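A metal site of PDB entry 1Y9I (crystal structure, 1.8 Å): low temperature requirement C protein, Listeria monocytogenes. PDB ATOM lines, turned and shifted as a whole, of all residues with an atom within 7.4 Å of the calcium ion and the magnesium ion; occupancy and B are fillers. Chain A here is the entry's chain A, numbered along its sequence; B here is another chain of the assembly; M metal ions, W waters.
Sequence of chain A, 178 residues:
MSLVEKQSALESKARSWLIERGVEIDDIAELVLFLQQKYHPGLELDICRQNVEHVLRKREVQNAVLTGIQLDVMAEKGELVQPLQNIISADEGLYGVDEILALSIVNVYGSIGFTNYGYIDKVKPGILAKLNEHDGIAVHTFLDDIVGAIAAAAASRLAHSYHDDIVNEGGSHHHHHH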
ATOM      1  N   ASP A  72      -7.343  -4.858 -14.219  1.00  0.00           N
ATOM      2  CA  ASP A  72      -5.884  -4.805 -14.048  1.00  0.00           C
ATOM      3  C   ASP A  72      -5.184  -5.473 -15.228  1.00  0.00           C
ATOM      4  O   ASP A  72      -4.220  -4.926 -15.798  1.00  0.00           O
ATOM      5  CB  ASP A  72      -5.444  -5.566 -12.795  1.00  0.00           C
ATOM      6  CG  ASP A  72      -5.777  -4.827 -11.519  1.00  0.00           C
ATOM      7  OD1 ASP A  72      -6.074  -3.618 -11.589  1.00  0.00           O
ATOM      8  OD2 ASP A  72      -5.727  -5.470 -10.445  1.00  0.00           O
ATOM      9  N   ASP A  91      -1.916   3.750 -11.717  1.00  0.00           N
ATOM     10  CA  ASP A  91      -2.510   3.801 -10.378  1.00  0.00           C
ATOM     11  C   ASP A  91      -2.671   5.248  -9.909  1.00  0.00           C
ATOM     12  O   ASP A  91      -2.277   5.599  -8.793  1.00  0.00           O
ATOM     13  CB  ASP A  91      -1.640   3.005  -9.401  1.00  0.00           C
ATOM     14  CG  ASP A  91      -2.331   2.757  -8.065  1.00  0.00           C
ATOM     15  OD1 ASP A  91      -3.527   3.092  -7.923  1.00  0.00           O
ATOM     16  OD2 ASP A  91      -1.660   2.216  -7.157  1.00  0.00           O
ATOM     17  N   GLU A  92      -3.248   6.085 -10.771  1.00  0.00           N
ATOM     18  CA  GLU A  92      -3.482   7.501 -10.487  1.00  0.00           C
ATOM     19  C   GLU A  92      -4.113   7.716  -9.125  1.00  0.00           C
ATOM     20  O   GLU A  92      -5.115   7.085  -8.784  1.00  0.00           O
ATOM     21  CB  GLU A  92      -4.399   8.090 -11.555  1.00  0.00           C
ATOM     22  CG  GLU A  92      -3.813   9.272 -12.302  1.00  0.00           C
ATOM     23  CD  GLU A  92      -4.774   9.833 -13.341  1.00  0.00           C
ATOM     24  OE1 GLU A  92      -5.893  10.257 -12.955  1.00  0.00           O
ATOM     25  OE2 GLU A  92      -4.403   9.863 -14.536  1.00  0.00           O
ATOM     26  N   GLY A  93      -3.521   8.622  -8.340  1.00  0.00           N
ATOM     27  CA  GLY A  93      -4.030   8.900  -7.015  1.00  0.00           C
ATOM     28  C   GLY A  93      -5.460   9.405  -6.935  1.00  0.00           C
ATOM     29  O   GLY A  93      -6.153   9.142  -5.952  1.00  0.00           O
ATOM     30  N   LEU A  94      -5.912  10.116  -7.962  1.00  0.00           N
ATOM     31  CA  LEU A  94      -7.280  10.641  -7.926  1.00  0.00           C
ATOM     32  C   LEU A  94      -8.321   9.709  -8.543  1.00  0.00           C
ATOM     33  O   LEU A  94      -9.501  10.077  -8.656  1.00  0.00           O
ATOM     34  CB  LEU A  94      -7.324  12.022  -8.586  1.00  0.00           C
ATOM     35  CG  LEU A  94      -6.417  13.059  -7.890  1.00  0.00           C
ATOM     36  CD1 LEU A  94      -6.619  14.427  -8.532  1.00  0.00           C
ATOM     37  CD2 LEU A  94      -6.743  13.131  -6.400  1.00  0.00           C
ATOM     38  N   TYR A  95      -7.909   8.515  -8.946  1.00  0.00           N
ATOM     39  CA  TYR A  95      -8.826   7.527  -9.500  1.00  0.00           C
ATOM     40  C   TYR A  95      -9.261   6.675  -8.304  1.00  0.00           C
ATOM     41  O   TYR A  95      -8.449   5.970  -7.701  1.00  0.00           O
ATOM     42  CB  TYR A  95      -8.118   6.659 -10.537  1.00  0.00           C
ATOM     43  CG  TYR A  95      -8.993   5.593 -11.164  1.00  0.00           C
ATOM     44  CD1 TYR A  95      -9.935   5.915 -12.148  1.00  0.00           C
ATOM     45  CD2 TYR A  95      -8.846   4.255 -10.792  1.00  0.00           C
ATOM     46  CE1 TYR A  95     -10.721   4.916 -12.749  1.00  0.00           C
ATOM     47  CE2 TYR A  95      -9.617   3.248 -11.397  1.00  0.00           C
ATOM     48  CZ  TYR A  95     -10.548   3.587 -12.369  1.00  0.00           C
ATOM     49  OH  TYR A  95     -11.286   2.572 -12.961  1.00  0.00           O
ATOM     50  N   GLY A  96     -10.539   6.738  -7.970  1.00  0.00           N
ATOM     51  CA  GLY A  96     -11.005   5.973  -6.816  1.00  0.00           C
ATOM     52  C   GLY A  96     -11.990   4.866  -7.093  1.00  0.00           C
ATOM     53  O   GLY A  96     -12.662   4.402  -6.177  1.00  0.00           O
ATOM     54  N   VAL A  97     -12.077   4.410  -8.340  1.00  0.00           N
ATOM     55  CA  VAL A  97     -13.017   3.348  -8.670  1.00  0.00           C
ATOM     56  C   VAL A  97     -12.560   2.034  -8.047  1.00  0.00           C
ATOM     57  O   VAL A  97     -13.389   1.209  -7.664  1.00  0.00           O
ATOM     58  CB  VAL A  97     -13.208   3.202 -10.204  1.00  0.00           C
ATOM     59  CG1 VAL A  97     -14.204   2.086 -10.505  1.00  0.00           C
ATOM     60  CG2 VAL A  97     -13.733   4.515 -10.788  1.00  0.00           C
ATOM     61  N   ASP A  98     -11.245   1.843  -7.903  1.00  0.00           N
ATOM     62  CA  ASP A  98     -10.735   0.615  -7.302  1.00  0.00           C
ATOM     63  C   ASP A  98     -11.108   0.544  -5.814  1.00  0.00           C
ATOM     64  O   ASP A  98     -11.420  -0.533  -5.309  1.00  0.00           O
ATOM     65  CB  ASP A  98      -9.197   0.474  -7.488  1.00  0.00           C
ATOM     66  CG  ASP A  98      -8.418   1.747  -7.188  1.00  0.00           C
ATOM     67  OD1 ASP A  98      -8.794   2.826  -7.680  1.00  0.00           O
ATOM     68  OD2 ASP A  98      -7.405   1.659  -6.449  1.00  0.00           O
ATOM     69  N   GLU A  99     -11.119   1.687  -5.138  1.00  0.00           N
ATOM     70  CA  GLU A  99     -11.488   1.729  -3.725  1.00  0.00           C
ATOM     71  C   GLU A  99     -13.002   1.508  -3.565  1.00  0.00           C
ATOM     72  O   GLU A  99     -13.467   0.933  -2.571  1.00  0.00           O
ATOM     73  CB  GLU A  99     -11.111   3.068  -3.098  1.00  0.00           C
ATOM     74  CG  GLU A  99      -9.601   3.271  -2.850  1.00  0.00           C
ATOM     75  CD  GLU A  99      -8.826   3.739  -4.083  1.00  0.00           C
ATOM     76  OE1 GLU A  99      -9.415   3.893  -5.164  1.00  0.00           O
ATOM     77  OE2 GLU A  99      -7.609   3.964  -3.956  1.00  0.00           O
ATOM     78  N   ILE A 100     -13.773   1.959  -4.543  1.00  0.00           N
ATOM     79  CA  ILE A 100     -15.232   1.800  -4.520  1.00  0.00           C
ATOM     80  C   ILE A 100     -15.612   0.335  -4.652  1.00  0.00           C
ATOM     81  O   ILE A 100     -16.425  -0.185  -3.889  1.00  0.00           O
ATOM     82  CB  ILE A 100     -15.892   2.610  -5.678  1.00  0.00           C
ATOM     83  CG1 ILE A 100     -15.877   4.101  -5.352  1.00  0.00           C
ATOM     84  CG2 ILE A 100     -17.292   2.114  -5.950  1.00  0.00           C
ATOM     85  CD1 ILE A 100     -16.755   4.486  -4.186  1.00  0.00           C
ATOM     86  N   TYR A 117      -9.945  -1.582   6.565  1.00  0.00           N
ATOM     87  CA  TYR A 117      -9.732  -1.516   5.125  1.00  0.00           C
ATOM     88  C   TYR A 117      -8.792  -0.342   4.810  1.00  0.00           C
ATOM     89  O   TYR A 117      -7.790  -0.509   4.106  1.00  0.00           O
ATOM     90  CB  TYR A 117     -11.076  -1.339   4.436  1.00  0.00           C
ATOM     91  CG  TYR A 117     -11.045  -1.029   2.956  1.00  0.00           C
ATOM     92  CD1 TYR A 117     -10.355  -1.850   2.058  1.00  0.00           C
ATOM     93  CD2 TYR A 117     -11.784   0.037   2.427  1.00  0.00           C
ATOM     94  CE1 TYR A 117     -10.404  -1.627   0.686  1.00  0.00           C
ATOM     95  CE2 TYR A 117     -11.840   0.271   1.063  1.00  0.00           C
ATOM     96  CZ  TYR A 117     -11.158  -0.558   0.194  1.00  0.00           C
ATOM     97  OH  TYR A 117     -11.254  -0.345  -1.162  1.00  0.00           O
ATOM     98  N   ASP A 121      -4.568  -0.541   3.889  1.00  0.00           N
ATOM     99  CA  ASP A 121      -4.189  -0.008   2.588  1.00  0.00           C
ATOM    100  C   ASP A 121      -3.013   0.956   2.726  1.00  0.00           C
ATOM    101  O   ASP A 121      -2.191   1.091   1.805  1.00  0.00           O
ATOM    102  CB  ASP A 121      -5.371   0.725   1.953  1.00  0.00           C
ATOM    103  CG  ASP A 121      -5.033   1.260   0.573  1.00  0.00           C
ATOM    104  OD1 ASP A 121      -4.778   0.431  -0.325  1.00  0.00           O
ATOM    105  OD2 ASP A 121      -5.013   2.500   0.392  1.00  0.00           O
ATOM    106  N   LYS A 124       0.169  -1.407   4.162  1.00  0.00           N
ATOM    107  CA  LYS A 124       0.558  -2.386   3.169  1.00  0.00           C
ATOM    108  C   LYS A 124       1.525  -3.463   3.666  1.00  0.00           C
ATOM    109  O   LYS A 124       2.619  -3.629   3.125  1.00  0.00           O
ATOM    110  CB  LYS A 124       1.169  -1.686   1.958  1.00  0.00           C
ATOM    111  CG  LYS A 124       0.252  -0.641   1.344  1.00  0.00           C
ATOM    112  CD  LYS A 124       0.883   0.049   0.152  1.00  0.00           C
ATOM    113  CE  LYS A 124      -0.057   1.094  -0.427  1.00  0.00           C
ATOM    114  NZ  LYS A 124      -1.342   0.491  -0.859  1.00  0.00           N
ATOM    115  N   HIS A 140      -1.683  -3.709 -10.488  1.00  0.00           N
ATOM    116  CA  HIS A 140      -2.474  -4.269  -9.402  1.00  0.00           C
ATOM    117  C   HIS A 140      -3.344  -3.188  -8.770  1.00  0.00           C
ATOM    118  O   HIS A 140      -3.645  -3.218  -7.581  1.00  0.00           O
ATOM    119  CB  HIS A 140      -1.554  -4.868  -8.331  1.00  0.00           C
ATOM    120  CG  HIS A 140      -0.770  -6.059  -8.812  1.00  0.00           C
ATOM    121  ND1 HIS A 140      -1.362  -7.264  -9.114  1.00  0.00           N
ATOM    122  CD2 HIS A 140       0.553  -6.222  -9.033  1.00  0.00           C
ATOM    123  CE1 HIS A 140      -0.433  -8.122  -9.503  1.00  0.00           C
ATOM    124  NE2 HIS A 140       0.734  -7.516  -9.468  1.00  0.00           N
ATOM    125  N   THR A 141      -3.735  -2.220  -9.599  1.00  0.00           N
ATOM    126  CA  THR A 141      -4.550  -1.105  -9.175  1.00  0.00           C
ATOM    127  C   THR A 141      -5.822  -1.554  -8.461  1.00  0.00           C
ATOM    128  O   THR A 141      -6.199  -0.991  -7.430  1.00  0.00           O
ATOM    129  CB  THR A 141      -4.913  -0.249 -10.400  1.00  0.00           C
ATOM    130  OG1 THR A 141      -3.705   0.276 -10.974  1.00  0.00           O
ATOM    131  CG2 THR A 141      -5.832   0.902 -10.008  1.00  0.00           C
ATOM    132  N   PHE A 142      -6.475  -2.582  -8.988  1.00  0.00           N
ATOM    133  CA  PHE A 142      -7.695  -3.090  -8.367  1.00  0.00           C
ATOM    134  C   PHE A 142      -7.427  -4.206  -7.364  1.00  0.00           C
ATOM    135  O   PHE A 142      -8.092  -4.298  -6.325  1.00  0.00           O
ATOM    136  CB  PHE A 142      -8.651  -3.603  -9.426  1.00  0.00           C
ATOM    137  CG  PHE A 142      -9.366  -2.520 -10.152  1.00  0.00           C
ATOM    138  CD1 PHE A 142     -10.609  -2.066  -9.697  1.00  0.00           C
ATOM    139  CD2 PHE A 142      -8.793  -1.918 -11.270  1.00  0.00           C
ATOM    140  CE1 PHE A 142     -11.250  -1.017 -10.338  1.00  0.00           C
ATOM    141  CE2 PHE A 142      -9.428  -0.856 -11.910  1.00  0.00           C
ATOM    142  CZ  PHE A 142     -10.663  -0.406 -11.441  1.00  0.00           C
ATOM    143  N   LEU A 143      -6.446  -5.049  -7.659  1.00  0.00           N
ATOM    144  CA  LEU A 143      -6.139  -6.160  -6.781  1.00  0.00           C
ATOM    145  C   LEU A 143      -5.649  -5.770  -5.388  1.00  0.00           C
ATOM    146  O   LEU A 143      -5.962  -6.463  -4.410  1.00  0.00           O
ATOM    147  CB  LEU A 143      -5.117  -7.092  -7.437  1.00  0.00           C
ATOM    148  CG  LEU A 143      -4.786  -8.351  -6.631  1.00  0.00           C
ATOM    149  CD1 LEU A 143      -6.070  -9.106  -6.307  1.00  0.00           C
ATOM    150  CD2 LEU A 143      -3.836  -9.248  -7.415  1.00  0.00           C
ATOM    151  N   ASP A 144      -4.883  -4.691  -5.264  1.00  0.00           N
ATOM    152  CA  ASP A 144      -4.426  -4.305  -3.936  1.00  0.00           C
ATOM    153  C   ASP A 144      -5.610  -3.996  -3.015  1.00  0.00           C
ATOM    154  O   ASP A 144      -5.614  -4.423  -1.855  1.00  0.00           O
ATOM    155  CB  ASP A 144      -3.423  -3.131  -3.960  1.00  0.00           C
ATOM    156  CG  ASP A 144      -3.880  -1.961  -4.793  1.00  0.00           C
ATOM    157  OD1 ASP A 144      -5.094  -1.803  -5.034  1.00  0.00           O
ATOM    158  OD2 ASP A 144      -3.001  -1.172  -5.217  1.00  0.00           O
ATOM    159  N   ASP A 145      -6.605  -3.273  -3.526  1.00  0.00           N
ATOM    160  CA  ASP A 145      -7.797  -2.935  -2.751  1.00  0.00           C
ATOM    161  C   ASP A 145      -8.589  -4.195  -2.446  1.00  0.00           C
ATOM    162  O   ASP A 145      -9.122  -4.369  -1.338  1.00  0.00           O
ATOM    163  CB  ASP A 145      -8.712  -1.990  -3.525  1.00  0.00           C
ATOM    164  CG  ASP A 145      -8.034  -0.695  -3.897  1.00  0.00           C
ATOM    165  OD1 ASP A 145      -7.845   0.151  -3.008  1.00  0.00           O
ATOM    166  OD2 ASP A 145      -7.694  -0.534  -5.085  1.00  0.00           O
ATOM    167  N   ILE A 146      -8.695  -5.082  -3.440  1.00  0.00           N
ATOM    168  CA  ILE A 146      -9.438  -6.324  -3.269  1.00  0.00           C
ATOM    169  C   ILE A 146      -8.872  -7.168  -2.132  1.00  0.00           C
ATOM    170  O   ILE A 146      -9.610  -7.667  -1.279  1.00  0.00           O
ATOM    171  CB  ILE A 146      -9.420  -7.139  -4.589  1.00  0.00           C
ATOM    172  CG1 ILE A 146     -10.345  -6.478  -5.615  1.00  0.00           C
ATOM    173  CG2 ILE A 146      -9.831  -8.576  -4.317  1.00  0.00           C
ATOM    174  CD1 ILE A 146     -10.262  -7.090  -7.029  1.00  0.00           C
ATOM    175  N   SER B 111     -14.171   8.561  -2.771  1.00  0.00           N
ATOM    176  CA  SER B 111     -13.601   7.340  -2.224  1.00  0.00           C
ATOM    177  C   SER B 111     -12.105   7.407  -1.944  1.00  0.00           C
ATOM    178  O   SER B 111     -11.585   6.586  -1.169  1.00  0.00           O
ATOM    179  CB  SER B 111     -13.869   6.175  -3.182  1.00  0.00           C
ATOM    180  OG  SER B 111     -13.382   6.508  -4.474  1.00  0.00           O
ATOM    181  N   ILE B 112     -11.401   8.346  -2.557  1.00  0.00           N
ATOM    182  CA  ILE B 112      -9.966   8.468  -2.328  1.00  0.00           C
ATOM    183  C   ILE B 112      -9.677   8.902  -0.885  1.00  0.00           C
ATOM    184  O   ILE B 112      -8.520   8.931  -0.449  1.00  0.00           O
ATOM    185  CB  ILE B 112      -9.305   9.474  -3.297  1.00  0.00           C
ATOM    186  CG1 ILE B 112      -9.939  10.858  -3.125  1.00  0.00           C
ATOM    187  CG2 ILE B 112      -9.459   8.976  -4.736  1.00  0.00           C
ATOM    188  CD1 ILE B 112      -9.319  11.924  -4.008  1.00  0.00           C
HETATM  189 CA    CA M   1      -7.308   4.306  -6.433  1.00  0.00          CA
HETATM  190 MG    MG M   2      -5.941   0.355  -5.937  1.00  0.00          MG
HETATM  191  O   HOH W   1      -5.879   4.394  -8.357  1.00  0.00           O
HETATM  192  O   HOH W   2      -5.881   1.205  -4.045  1.00  0.00           O
HETATM  193  O   HOH W   3      -4.056   0.867  -6.269  1.00  0.00           O
HETATM  194  O   HOH W   4      -6.513   6.401  -5.401  1.00  0.00           O
HETATM  195  O   HOH W   5      -5.080   3.578  -5.507  1.00  0.00           O
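Water W3 is bound to the magnesium ion, 2.0 Å away.
The backbone carbonyl oxygen (O) of Thr 141 is bound to the magnesium ion, 2.0 Å away.
OD2 of Asp 98 binds the magnesium ion, at 2.0 Å.
The magnesium ion is bound by water W2, 2.1 Å away.
The magnesium ion is bound by OD2 of Asp 145 (2.1 Å).
The magnesium ion is bound by OD1 of Asp 144 (2.5 Å).
The magnesium ion has six donor atoms within binding distance.
The backbone NH of Thr 141 lies within hydrogen-bond range of the side-chain carboxylate of Asp 72 (3.4 Å).
O of Glu 99 sits at hydrogen-bond distance from OH of Tyr 117 (2.9 Å).
Three residues have an atom within 4 Å of the calcium ion: Tyr 95, Asp 98 and Glu 99.
Water W1 bridges OD1 of Asp 91 and O of Glu 92.
Water W3 bridges the side-chain carboxylate of Asp 144 (2.5 Å) and the side-chain carboxylate of Asp 91 (2.8 Å).
The calcium ion is bound by the backbone carbonyl oxygen (O) of Tyr 95.
Water W1 binds the calcium ion (2.4 Å).
The calcium ion is bound by OD1 of Asp 98, at 2.4 Å.
The calcium ion is bound by water W4, 2.5 Å away.
The calcium ion is bound by the side-chain carboxylate (OE1) of Glu 99 (2.5 Å).
OE2 of Glu 99 is bound to the calcium ion.
The calcium ion is bound by water W5 (2.5 Å).
The calcium ion is bound by OD2 of Asp 98, at 2.6 Å.
The calcium ion has eight donor atoms within binding distance.
Within 4 Å of the magnesium ion: Asp 98, Thr 141, Asp 144 and Asp 145.
The nearest printed residue that does not touch the magnesium ion is Asp 91 (4.2 Å).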
